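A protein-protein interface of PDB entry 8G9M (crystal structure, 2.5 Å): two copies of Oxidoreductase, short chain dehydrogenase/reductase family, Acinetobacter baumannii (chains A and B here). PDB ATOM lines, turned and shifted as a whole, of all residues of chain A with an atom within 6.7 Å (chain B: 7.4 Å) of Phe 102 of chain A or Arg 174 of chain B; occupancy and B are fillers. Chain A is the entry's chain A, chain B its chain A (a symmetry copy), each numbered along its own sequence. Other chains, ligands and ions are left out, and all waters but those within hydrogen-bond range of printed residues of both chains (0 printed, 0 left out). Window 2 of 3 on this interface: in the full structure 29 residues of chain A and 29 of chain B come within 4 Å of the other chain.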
ATOM      1  N   GLU A  99      -3.916 -36.209  -3.231  1.00  0.00           N
ATOM      2  CA  GLU A  99      -4.281 -35.483  -4.439  1.00  0.00           C
ATOM      3  C   GLU A  99      -3.785 -34.044  -4.364  1.00  0.00           C
ATOM      4  O   GLU A  99      -3.876 -33.393  -3.319  1.00  0.00           O
ATOM      5  CB  GLU A  99      -5.796 -35.512  -4.639  1.00  0.00           C
ATOM      6  CG  GLU A  99      -6.324 -36.833  -5.171  1.00  0.00           C
ATOM      7  CD  GLU A  99      -5.687 -37.221  -6.491  1.00  0.00           C
ATOM      8  OE1 GLU A  99      -4.765 -38.064  -6.483  1.00  0.00           O
ATOM      9  OE2 GLU A  99      -6.108 -36.681  -7.537  1.00  0.00           O
ATOM     10  N   ASP A 100      -3.250 -33.552  -5.481  1.00  0.00           N
ATOM     11  CA  ASP A 100      -2.734 -32.191  -5.521  1.00  0.00           C
ATOM     12  C   ASP A 100      -3.852 -31.191  -5.255  1.00  0.00           C
ATOM     13  O   ASP A 100      -5.002 -31.394  -5.661  1.00  0.00           O
ATOM     14  CB  ASP A 100      -2.081 -31.909  -6.874  1.00  0.00           C
ATOM     15  CG  ASP A 100      -1.339 -30.586  -6.898  1.00  0.00           C
ATOM     16  OD1 ASP A 100      -0.279 -30.482  -6.245  1.00  0.00           O
ATOM     17  OD2 ASP A 100      -1.823 -29.649  -7.567  1.00  0.00           O
ATOM     18  N   PHE A 101      -3.501 -30.102  -4.563  1.00  0.00           N
ATOM     19  CA  PHE A 101      -4.502 -29.139  -4.114  1.00  0.00           C
ATOM     20  C   PHE A 101      -5.320 -28.597  -5.278  1.00  0.00           C
ATOM     21  O   PHE A 101      -6.528 -28.371  -5.145  1.00  0.00           O
ATOM     22  CB  PHE A 101      -3.818 -27.995  -3.363  1.00  0.00           C
ATOM     23  CG  PHE A 101      -4.710 -26.810  -3.118  1.00  0.00           C
ATOM     24  CD1 PHE A 101      -5.545 -26.776  -2.016  1.00  0.00           C
ATOM     25  CD2 PHE A 101      -4.710 -25.726  -3.988  1.00  0.00           C
ATOM     26  CE1 PHE A 101      -6.369 -25.688  -1.782  1.00  0.00           C
ATOM     27  CE2 PHE A 101      -5.534 -24.635  -3.763  1.00  0.00           C
ATOM     28  CZ  PHE A 101      -6.362 -24.615  -2.658  1.00  0.00           C
ATOM     29  N   PHE A 102      -4.680 -28.374  -6.424  1.00  0.00           N
ATOM     30  CA  PHE A 102      -5.371 -27.779  -7.559  1.00  0.00           C
ATOM     31  C   PHE A 102      -6.151 -28.794  -8.379  1.00  0.00           C
ATOM     32  O   PHE A 102      -6.865 -28.398  -9.305  1.00  0.00           O
ATOM     33  CB  PHE A 102      -4.368 -27.038  -8.447  1.00  0.00           C
ATOM     34  CG  PHE A 102      -3.648 -25.928  -7.737  1.00  0.00           C
ATOM     35  CD1 PHE A 102      -2.341 -26.092  -7.312  1.00  0.00           C
ATOM     36  CD2 PHE A 102      -4.290 -24.731  -7.469  1.00  0.00           C
ATOM     37  CE1 PHE A 102      -1.682 -25.076  -6.646  1.00  0.00           C
ATOM     38  CE2 PHE A 102      -3.638 -23.714  -6.804  1.00  0.00           C
ATOM     39  CZ  PHE A 102      -2.332 -23.886  -6.392  1.00  0.00           C
ATOM     40  N   SER A 103      -6.044 -30.084  -8.059  1.00  0.00           N
ATOM     41  CA  SER A 103      -6.819 -31.108  -8.744  1.00  0.00           C
ATOM     42  C   SER A 103      -8.018 -31.590  -7.938  1.00  0.00           C
ATOM     43  O   SER A 103      -8.982 -32.085  -8.532  1.00  0.00           O
ATOM     44  CB  SER A 103      -5.927 -32.307  -9.090  1.00  0.00           C
ATOM     45  OG  SER A 103      -5.627 -33.070  -7.934  1.00  0.00           O
ATOM     46  N   VAL A 104      -7.988 -31.447  -6.617  1.00  0.00           N
ATOM     47  CA  VAL A 104      -9.067 -31.928  -5.757  1.00  0.00           C
ATOM     48  C   VAL A 104     -10.249 -30.969  -5.843  1.00  0.00           C
ATOM     49  O   VAL A 104     -10.097 -29.767  -5.579  1.00  0.00           O
ATOM     50  CB  VAL A 104      -8.580 -32.118  -4.308  1.00  0.00           C
ATOM     51  CG1 VAL A 104      -7.802 -30.911  -3.839  1.00  0.00           C
ATOM     52  CG2 VAL A 104      -9.749 -32.359  -3.382  1.00  0.00           C
ATOM     53  N   PRO A 105     -11.439 -31.451  -6.225  1.00  0.00           N
ATOM     54  CA  PRO A 105     -12.589 -30.550  -6.386  1.00  0.00           C
ATOM     55  C   PRO A 105     -13.358 -30.305  -5.096  1.00  0.00           C
ATOM     56  O   PRO A 105     -13.011 -30.849  -4.042  1.00  0.00           O
ATOM     57  CB  PRO A 105     -13.455 -31.284  -7.417  1.00  0.00           C
ATOM     58  CG  PRO A 105     -13.163 -32.720  -7.174  1.00  0.00           C
ATOM     59  CD  PRO A 105     -11.724 -32.808  -6.720  1.00  0.00           C
ATOM     60  N   PRO A 151       1.111 -30.749   5.616  1.00  0.00           N
ATOM     61  CA  PRO A 151       2.285 -31.088   4.786  1.00  0.00           C
ATOM     62  C   PRO A 151       2.448 -30.232   3.540  1.00  0.00           C
ATOM     63  O   PRO A 151       3.549 -29.729   3.283  1.00  0.00           O
ATOM     64  CB  PRO A 151       2.038 -32.565   4.442  1.00  0.00           C
ATOM     65  CG  PRO A 151       1.140 -33.059   5.532  1.00  0.00           C
ATOM     66  CD  PRO A 151       0.235 -31.911   5.835  1.00  0.00           C
ATOM     67  N   GLY A 152       1.390 -30.059   2.745  1.00  0.00           N
ATOM     68  CA  GLY A 152       1.452 -29.316   1.496  1.00  0.00           C
ATOM     69  C   GLY A 152       1.142 -30.162   0.276  1.00  0.00           C
ATOM     70  O   GLY A 152       0.624 -29.643  -0.717  1.00  0.00           O
ATOM     71  N   ASP A 153       1.466 -31.452   0.328  1.00  0.00           N
ATOM     72  CA  ASP A 153       1.016 -32.412  -0.670  1.00  0.00           C
ATOM     73  C   ASP A 153      -0.197 -33.201  -0.199  1.00  0.00           C
ATOM     74  O   ASP A 153      -0.732 -34.012  -0.962  1.00  0.00           O
ATOM     75  CB  ASP A 153       2.156 -33.372  -1.035  1.00  0.00           C
ATOM     76  CG  ASP A 153       2.827 -33.972   0.184  1.00  0.00           C
ATOM     77  OD1 ASP A 153       3.677 -34.873   0.013  1.00  0.00           O
ATOM     78  OD2 ASP A 153       2.510 -33.543   1.312  1.00  0.00           O
ATOM     79  N   ILE A 155      -3.034 -31.536   1.659  1.00  0.00           N
ATOM     80  CA  ILE A 155      -3.638 -30.378   2.312  1.00  0.00           C
ATOM     81  C   ILE A 155      -5.017 -30.718   2.865  1.00  0.00           C
ATOM     82  O   ILE A 155      -5.360 -30.326   3.987  1.00  0.00           O
ATOM     83  CB  ILE A 155      -3.694 -29.189   1.336  1.00  0.00           C
ATOM     84  CG1 ILE A 155      -2.315 -28.956   0.711  1.00  0.00           C
ATOM     85  CG2 ILE A 155      -4.181 -27.932   2.047  1.00  0.00           C
ATOM     86  CD1 ILE A 155      -2.161 -27.614   0.025  1.00  0.00           C
ATOM     87  N   VAL B 121     -10.970 -21.747  -0.408  1.00  0.00           N
ATOM     88  CA  VAL B 121     -10.263 -22.761  -1.185  1.00  0.00           C
ATOM     89  C   VAL B 121     -10.553 -22.589  -2.669  1.00  0.00           C
ATOM     90  O   VAL B 121      -9.655 -22.703  -3.507  1.00  0.00           O
ATOM     91  CB  VAL B 121     -10.639 -24.172  -0.694  1.00  0.00           C
ATOM     92  CG1 VAL B 121     -10.118 -25.229  -1.658  1.00  0.00           C
ATOM     93  CG2 VAL B 121     -10.098 -24.410   0.710  1.00  0.00           C
ATOM     94  N   ALA B 124      -8.703 -19.416  -3.959  1.00  0.00           N
ATOM     95  CA  ALA B 124      -7.271 -19.681  -4.052  1.00  0.00           C
ATOM     96  C   ALA B 124      -6.959 -20.616  -5.211  1.00  0.00           C
ATOM     97  O   ALA B 124      -6.036 -20.359  -5.992  1.00  0.00           O
ATOM     98  CB  ALA B 124      -6.759 -20.261  -2.734  1.00  0.00           C
ATOM     99  N   ARG B 125      -7.723 -21.705  -5.343  1.00  0.00           N
ATOM    100  CA  ARG B 125      -7.520 -22.643  -6.438  1.00  0.00           C
ATOM    101  C   ARG B 125      -7.624 -21.955  -7.789  1.00  0.00           C
ATOM    102  O   ARG B 125      -6.919 -22.333  -8.732  1.00  0.00           O
ATOM    103  CB  ARG B 125      -8.542 -23.779  -6.342  1.00  0.00           C
ATOM    104  CG  ARG B 125      -8.425 -24.837  -7.430  1.00  0.00           C
ATOM    105  CD  ARG B 125      -9.252 -26.072  -7.093  1.00  0.00           C
ATOM    106  NE  ARG B 125     -10.686 -25.802  -7.134  1.00  0.00           N
ATOM    107  CZ  ARG B 125     -11.524 -26.047  -6.131  1.00  0.00           C
ATOM    108  NH1 ARG B 125     -11.073 -26.573  -5.001  1.00  0.00           N
ATOM    109  NH2 ARG B 125     -12.814 -25.766  -6.259  1.00  0.00           N
ATOM    110  N   HIS B 126      -8.487 -20.945  -7.906  1.00  0.00           N
ATOM    111  CA  HIS B 126      -8.598 -20.273  -9.197  1.00  0.00           C
ATOM    112  C   HIS B 126      -7.479 -19.260  -9.422  1.00  0.00           C
ATOM    113  O   HIS B 126      -6.920 -19.194 -10.522  1.00  0.00           O
ATOM    114  CB  HIS B 126      -9.948 -19.580  -9.342  1.00  0.00           C
ATOM    115  CG  HIS B 126     -10.104 -18.853 -10.643  1.00  0.00           C
ATOM    116  ND1 HIS B 126     -10.123 -17.478 -10.730  1.00  0.00           N
ATOM    117  CD2 HIS B 126     -10.233 -19.310 -11.911  1.00  0.00           C
ATOM    118  CE1 HIS B 126     -10.266 -17.119 -11.993  1.00  0.00           C
ATOM    119  NE2 HIS B 126     -10.335 -18.212 -12.731  1.00  0.00           N
ATOM    120  N   TYR B 127      -7.139 -18.460  -8.408  1.00  0.00           N
ATOM    121  CA  TYR B 127      -6.238 -17.334  -8.637  1.00  0.00           C
ATOM    122  C   TYR B 127      -4.759 -17.669  -8.472  1.00  0.00           C
ATOM    123  O   TYR B 127      -3.918 -16.928  -8.995  1.00  0.00           O
ATOM    124  CB  TYR B 127      -6.592 -16.174  -7.702  1.00  0.00           C
ATOM    125  CG  TYR B 127      -7.858 -15.450  -8.090  1.00  0.00           C
ATOM    126  CD1 TYR B 127      -7.984 -14.843  -9.334  1.00  0.00           C
ATOM    127  CD2 TYR B 127      -8.930 -15.373  -7.213  1.00  0.00           C
ATOM    128  CE1 TYR B 127      -9.143 -14.179  -9.692  1.00  0.00           C
ATOM    129  CE2 TYR B 127     -10.092 -14.712  -7.560  1.00  0.00           C
ATOM    130  CZ  TYR B 127     -10.193 -14.116  -8.801  1.00  0.00           C
ATOM    131  OH  TYR B 127     -11.351 -13.458  -9.147  1.00  0.00           O
ATOM    132  N   ALA B 128      -4.415 -18.752  -7.778  1.00  0.00           N
ATOM    133  CA  ALA B 128      -3.020 -19.093  -7.517  1.00  0.00           C
ATOM    134  C   ALA B 128      -2.197 -19.430  -8.763  1.00  0.00           C
ATOM    135  O   ALA B 128      -1.014 -19.069  -8.812  1.00  0.00           O
ATOM    136  CB  ALA B 128      -2.956 -20.258  -6.526  1.00  0.00           C
ATOM    137  N   PRO B 129      -2.742 -20.136  -9.770  1.00  0.00           N
ATOM    138  CA  PRO B 129      -1.887 -20.521 -10.912  1.00  0.00           C
ATOM    139  C   PRO B 129      -1.299 -19.345 -11.674  1.00  0.00           C
ATOM    140  O   PRO B 129      -0.117 -19.382 -12.037  1.00  0.00           O
ATOM    141  CB  PRO B 129      -2.834 -21.352 -11.790  1.00  0.00           C
ATOM    142  CG  PRO B 129      -3.850 -21.874 -10.852  1.00  0.00           C
ATOM    143  CD  PRO B 129      -4.066 -20.779  -9.859  1.00  0.00           C
ATOM    144  N   VAL B 132       1.505 -17.927  -9.715  1.00  0.00           N
ATOM    145  CA  VAL B 132       2.697 -18.757  -9.843  1.00  0.00           C
ATOM    146  C   VAL B 132       3.358 -18.536 -11.196  1.00  0.00           C
ATOM    147  O   VAL B 132       4.591 -18.562 -11.307  1.00  0.00           O
ATOM    148  CB  VAL B 132       2.330 -20.238  -9.622  1.00  0.00           C
ATOM    149  CG1 VAL B 132       3.520 -21.140  -9.907  1.00  0.00           C
ATOM    150  CG2 VAL B 132       1.823 -20.452  -8.208  1.00  0.00           C
ATOM    151  N   ILE B 139      -1.490 -14.447  -1.046  1.00  0.00           N
ATOM    152  CA  ILE B 139      -2.766 -15.018  -0.627  1.00  0.00           C
ATOM    153  C   ILE B 139      -2.839 -14.925   0.892  1.00  0.00           C
ATOM    154  O   ILE B 139      -1.954 -15.434   1.591  1.00  0.00           O
ATOM    155  CB  ILE B 139      -2.935 -16.473  -1.097  1.00  0.00           C
ATOM    156  CG1 ILE B 139      -2.721 -16.574  -2.610  1.00  0.00           C
ATOM    157  CG2 ILE B 139      -4.313 -16.997  -0.720  1.00  0.00           C
ATOM    158  CD1 ILE B 139      -2.666 -17.996  -3.133  1.00  0.00           C
ATOM    159  N   SER B 168      -4.078 -22.298   4.824  1.00  0.00           N
ATOM    160  CA  SER B 168      -3.052 -21.326   4.457  1.00  0.00           C
ATOM    161  C   SER B 168      -1.654 -21.897   4.683  1.00  0.00           C
ATOM    162  O   SER B 168      -0.764 -21.720   3.846  1.00  0.00           O
ATOM    163  CB  SER B 168      -3.225 -20.033   5.248  1.00  0.00           C
ATOM    164  OG  SER B 168      -2.339 -19.972   6.350  1.00  0.00           O
ATOM    165  N   HIS B 169      -1.444 -22.602   5.798  1.00  0.00           N
ATOM    166  CA  HIS B 169      -0.151 -23.237   6.049  1.00  0.00           C
ATOM    167  C   HIS B 169       0.200 -24.231   4.942  1.00  0.00           C
ATOM    168  O   HIS B 169       1.307 -24.201   4.377  1.00  0.00           O
ATOM    169  CB  HIS B 169      -0.193 -23.922   7.412  1.00  0.00           C
ATOM    170  CG  HIS B 169       1.157 -24.179   8.005  1.00  0.00           C
ATOM    171  ND1 HIS B 169       2.120 -24.938   7.375  1.00  0.00           N
ATOM    172  CD2 HIS B 169       1.695 -23.794   9.185  1.00  0.00           C
ATOM    173  CE1 HIS B 169       3.197 -25.005   8.140  1.00  0.00           C
ATOM    174  NE2 HIS B 169       2.965 -24.317   9.243  1.00  0.00           N
ATOM    175  N   GLY B 170      -0.741 -25.118   4.614  1.00  0.00           N
ATOM    176  CA  GLY B 170      -0.471 -26.141   3.619  1.00  0.00           C
ATOM    177  C   GLY B 170      -0.256 -25.575   2.229  1.00  0.00           C
ATOM    178  O   GLY B 170       0.651 -26.006   1.511  1.00  0.00           O
ATOM    179  N   LEU B 171      -1.081 -24.605   1.822  1.00  0.00           N
ATOM    180  CA  LEU B 171      -0.888 -24.026   0.499  1.00  0.00           C
ATOM    181  C   LEU B 171       0.378 -23.183   0.448  1.00  0.00           C
ATOM    182  O   LEU B 171       0.992 -23.063  -0.618  1.00  0.00           O
ATOM    183  CB  LEU B 171      -2.101 -23.194   0.081  1.00  0.00           C
ATOM    184  CG  LEU B 171      -2.120 -22.830  -1.410  1.00  0.00           C
ATOM    185  CD1 LEU B 171      -1.667 -24.008  -2.263  1.00  0.00           C
ATOM    186  CD2 LEU B 171      -3.495 -22.355  -1.845  1.00  0.00           C
ATOM    187  N   ALA B 172       0.805 -22.614   1.578  1.00  0.00           N
ATOM    188  CA  ALA B 172       2.101 -21.954   1.611  1.00  0.00           C
ATOM    189  C   ALA B 172       3.214 -22.945   1.315  1.00  0.00           C
ATOM    190  O   ALA B 172       4.073 -22.696   0.461  1.00  0.00           O
ATOM    191  CB  ALA B 172       2.317 -21.296   2.965  1.00  0.00           C
ATOM    192  N   LYS B 173       3.212 -24.083   2.014  1.00  0.00           N
ATOM    193  CA  LYS B 173       4.224 -25.101   1.736  1.00  0.00           C
ATOM    194  C   LYS B 173       4.138 -25.586   0.290  1.00  0.00           C
ATOM    195  O   LYS B 173       5.166 -25.838  -0.350  1.00  0.00           O
ATOM    196  CB  LYS B 173       4.084 -26.268   2.712  1.00  0.00           C
ATOM    197  CG  LYS B 173       4.831 -26.041   4.015  1.00  0.00           C
ATOM    198  CD  LYS B 173       5.155 -27.341   4.724  1.00  0.00           C
ATOM    199  CE  LYS B 173       4.570 -27.348   6.127  1.00  0.00           C
ATOM    200  NZ  LYS B 173       5.341 -28.206   7.066  1.00  0.00           N
ATOM    201  N   ARG B 174       2.921 -25.696  -0.244  1.00  0.00           N
ATOM    202  CA  ARG B 174       2.743 -26.184  -1.609  1.00  0.00           C
ATOM    203  C   ARG B 174       3.264 -25.184  -2.636  1.00  0.00           C
ATOM    204  O   ARG B 174       3.825 -25.579  -3.666  1.00  0.00           O
ATOM    205  CB  ARG B 174       1.264 -26.494  -1.852  1.00  0.00           C
ATOM    206  CG  ARG B 174       0.848 -26.553  -3.312  1.00  0.00           C
ATOM    207  CD  ARG B 174       1.396 -27.788  -4.005  1.00  0.00           C
ATOM    208  NE  ARG B 174       0.841 -27.940  -5.345  1.00  0.00           N
ATOM    209  CZ  ARG B 174       1.346 -27.362  -6.429  1.00  0.00           C
ATOM    210  NH1 ARG B 174       2.418 -26.589  -6.328  1.00  0.00           N
ATOM    211  NH2 ARG B 174       0.778 -27.552  -7.613  1.00  0.00           N
ATOM    212  N   LEU B 175       3.094 -23.890  -2.374  1.00  0.00           N
ATOM    213  CA  LEU B 175       3.529 -22.837  -3.282  1.00  0.00           C
ATOM    214  C   LEU B 175       4.921 -22.314  -2.956  1.00  0.00           C
ATOM    215  O   LEU B 175       5.363 -21.339  -3.574  1.00  0.00           O
ATOM    216  CB  LEU B 175       2.528 -21.679  -3.268  1.00  0.00           C
ATOM    217  CG  LEU B 175       1.125 -21.990  -3.788  1.00  0.00           C
ATOM    218  CD1 LEU B 175       0.193 -20.810  -3.562  1.00  0.00           C
ATOM    219  CD2 LEU B 175       1.174 -22.371  -5.256  1.00  0.00           C
ATOM    220  N   ALA B 176       5.613 -22.930  -2.000  1.00  0.00           N
ATOM    221  CA  ALA B 176       6.978 -22.530  -1.687  1.00  0.00           C
ATOM    222  C   ALA B 176       7.876 -22.711  -2.905  1.00  0.00           C
ATOM    223  O   ALA B 176       7.676 -23.610  -3.725  1.00  0.00           O
ATOM    224  CB  ALA B 176       7.515 -23.341  -0.509  1.00  0.00           C
ATOM    225  N   GLY B 177       8.877 -21.840  -3.019  1.00  0.00           N
ATOM    226  CA  GLY B 177       9.740 -21.798  -4.174  1.00  0.00           C
ATOM    227  C   GLY B 177       9.245 -20.887  -5.279  1.00  0.00           C
ATOM    228  O   GLY B 177      10.059 -20.303  -6.002  1.00  0.00           O
ATOM    229  N   THR B 178       7.929 -20.757  -5.430  1.00  0.00           N
ATOM    230  CA  THR B 178       7.362 -19.769  -6.329  1.00  0.00           C
ATOM    231  C   THR B 178       7.405 -18.395  -5.666  1.00  0.00           C
ATOM    232  O   THR B 178       7.860 -18.237  -4.529  1.00  0.00           O
ATOM    233  CB  THR B 178       5.932 -20.150  -6.711  1.00  0.00           C
ATOM    234  OG1 THR B 178       5.035 -19.777  -5.658  1.00  0.00           O
ATOM    235  CG2 THR B 178       5.826 -21.647  -6.950  1.00  0.00           C
ATOM    236  N   VAL B 180       4.759 -16.785  -4.818  1.00  0.00           N
ATOM    237  CA  VAL B 180       3.494 -16.637  -4.110  1.00  0.00           C
ATOM    238  C   VAL B 180       3.707 -17.000  -2.650  1.00  0.00           C
ATOM    239  O   VAL B 180       4.258 -18.063  -2.339  1.00  0.00           O
ATOM    240  CB  VAL B 180       2.402 -17.519  -4.735  1.00  0.00           C
ATOM    241  CG1 VAL B 180       1.035 -17.116  -4.210  1.00  0.00           C
ATOM    242  CG2 VAL B 180       2.454 -17.425  -6.249  1.00  0.00           C
ATOM    243  N   VAL B 182       1.620 -17.448   1.092  1.00  0.00           N
ATOM    244  CA  VAL B 182       0.316 -17.668   1.703  1.00  0.00           C
ATOM    245  C   VAL B 182       0.473 -17.461   3.201  1.00  0.00           C
ATOM    246  O   VAL B 182       1.317 -18.103   3.837  1.00  0.00           O
ATOM    247  CB  VAL B 182      -0.234 -19.069   1.393  1.00  0.00           C
ATOM    248  CG1 VAL B 182      -1.652 -19.207   1.927  1.00  0.00           C
ATOM    249  CG2 VAL B 182      -0.186 -19.347  -0.106  1.00  0.00           C
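The guanidinium group (NE) of Arg 174 of chain B is in salt-bridge range of the side-chain carboxylate (OD1) of Asp 100 of chain A, at 2.9 Å.
The backbone carbonyl oxygen (O) of Val 104 of chain A is in hydrogen-bond range of the guanidinium group (NH1) of Arg 125 of chain B (3.4 Å).
N of Phe 102 of chain A sits close to OD2 of Asp 100 of chain A.
OG of Ser 103 of chain A lies within hydrogen-bond range of O of Asp 100 of chain A, at 2.9 Å.
O of Leu 175 of chain B sits at hydrogen-bond distance from OG1 of Thr 178 of chain B (2.6 Å).
Among the printed residues, pairs that only touch across the chains: Phe 101 of chain A with Val 121 of chain B (3.8 Å), Phe 101 of chain A with Arg 125 of chain B (3.9 Å), Phe 101 of chain A with Leu 171 of chain B (3.6 Å), Phe 102 of chain A with Arg 125 of chain B (3.8 Å), Phe 102 of chain A with Ala 128 of chain B (3.5 Å), Phe 102 of chain A with Arg 174 of chain B (3.5 Å), Phe 102 of chain A with Leu 175 of chain B (3.98 Å), Pro 151 of chain A with Lys 173 of chain B (3.2 Å), Gly 152 of chain A with Gly 170 of chain B (3.4 Å), Gly 152 of chain A with Arg 174 of chain B (3.4 Å), Ile 155 of chain A with Gly 170 of chain B (3.6 Å) and Ile 155 of chain A with Leu 171 of chain B (3.7 Å).
Of the printed residues of chain B, Phe 102 of chain A touches Arg 125, Ala 128, Arg 174 and Leu 175.
Arg 174 of chain B touches three residues of chain A.
Of the printed residues of chain A, Gly 170 of chain B touches Gly 152 and Ile 155.
Of the printed residues of chain A, Leu 175 of chain B touches Phe 102 (3.98 Å).
Of the printed residues of chain B, Val 104 of chain A touches Arg 125 (3.4 Å).
Of the printed residues of chain A, Arg 125 of chain B touches Phe 101 (3.9 Å), Phe 102 (3.8 Å) and Val 104 (3.4 Å).
Thr 178 of chain B touches none of the printed residues of chain A.
Printed residues of chain A that touch a printed residue of chain B: Asp 100, Phe 101, Phe 102, Val 104, Pro 151, Gly 152 and Ile 155.
Of the 22 printed residues of chain B, 8 touch a printed residue of chain A.
Printed residues of chain B that touch a printed residue of chain A: Val 121, Arg 125, Ala 128, Gly 170, Leu 171, Lys 173, Arg 174 and Leu 175.
Hydrophobic or aromatic side chains of chain B within 4 Å of the printed part of chain A: Val 121, Ala 128, Leu 171 and Leu 175.
Among the printed residues, 14 pairs touch across the chains.
No position is printed for both chains.
Of the 14 pairs that touch across the chains among the printed residues, none has its exchanged pair printed and touching as well.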
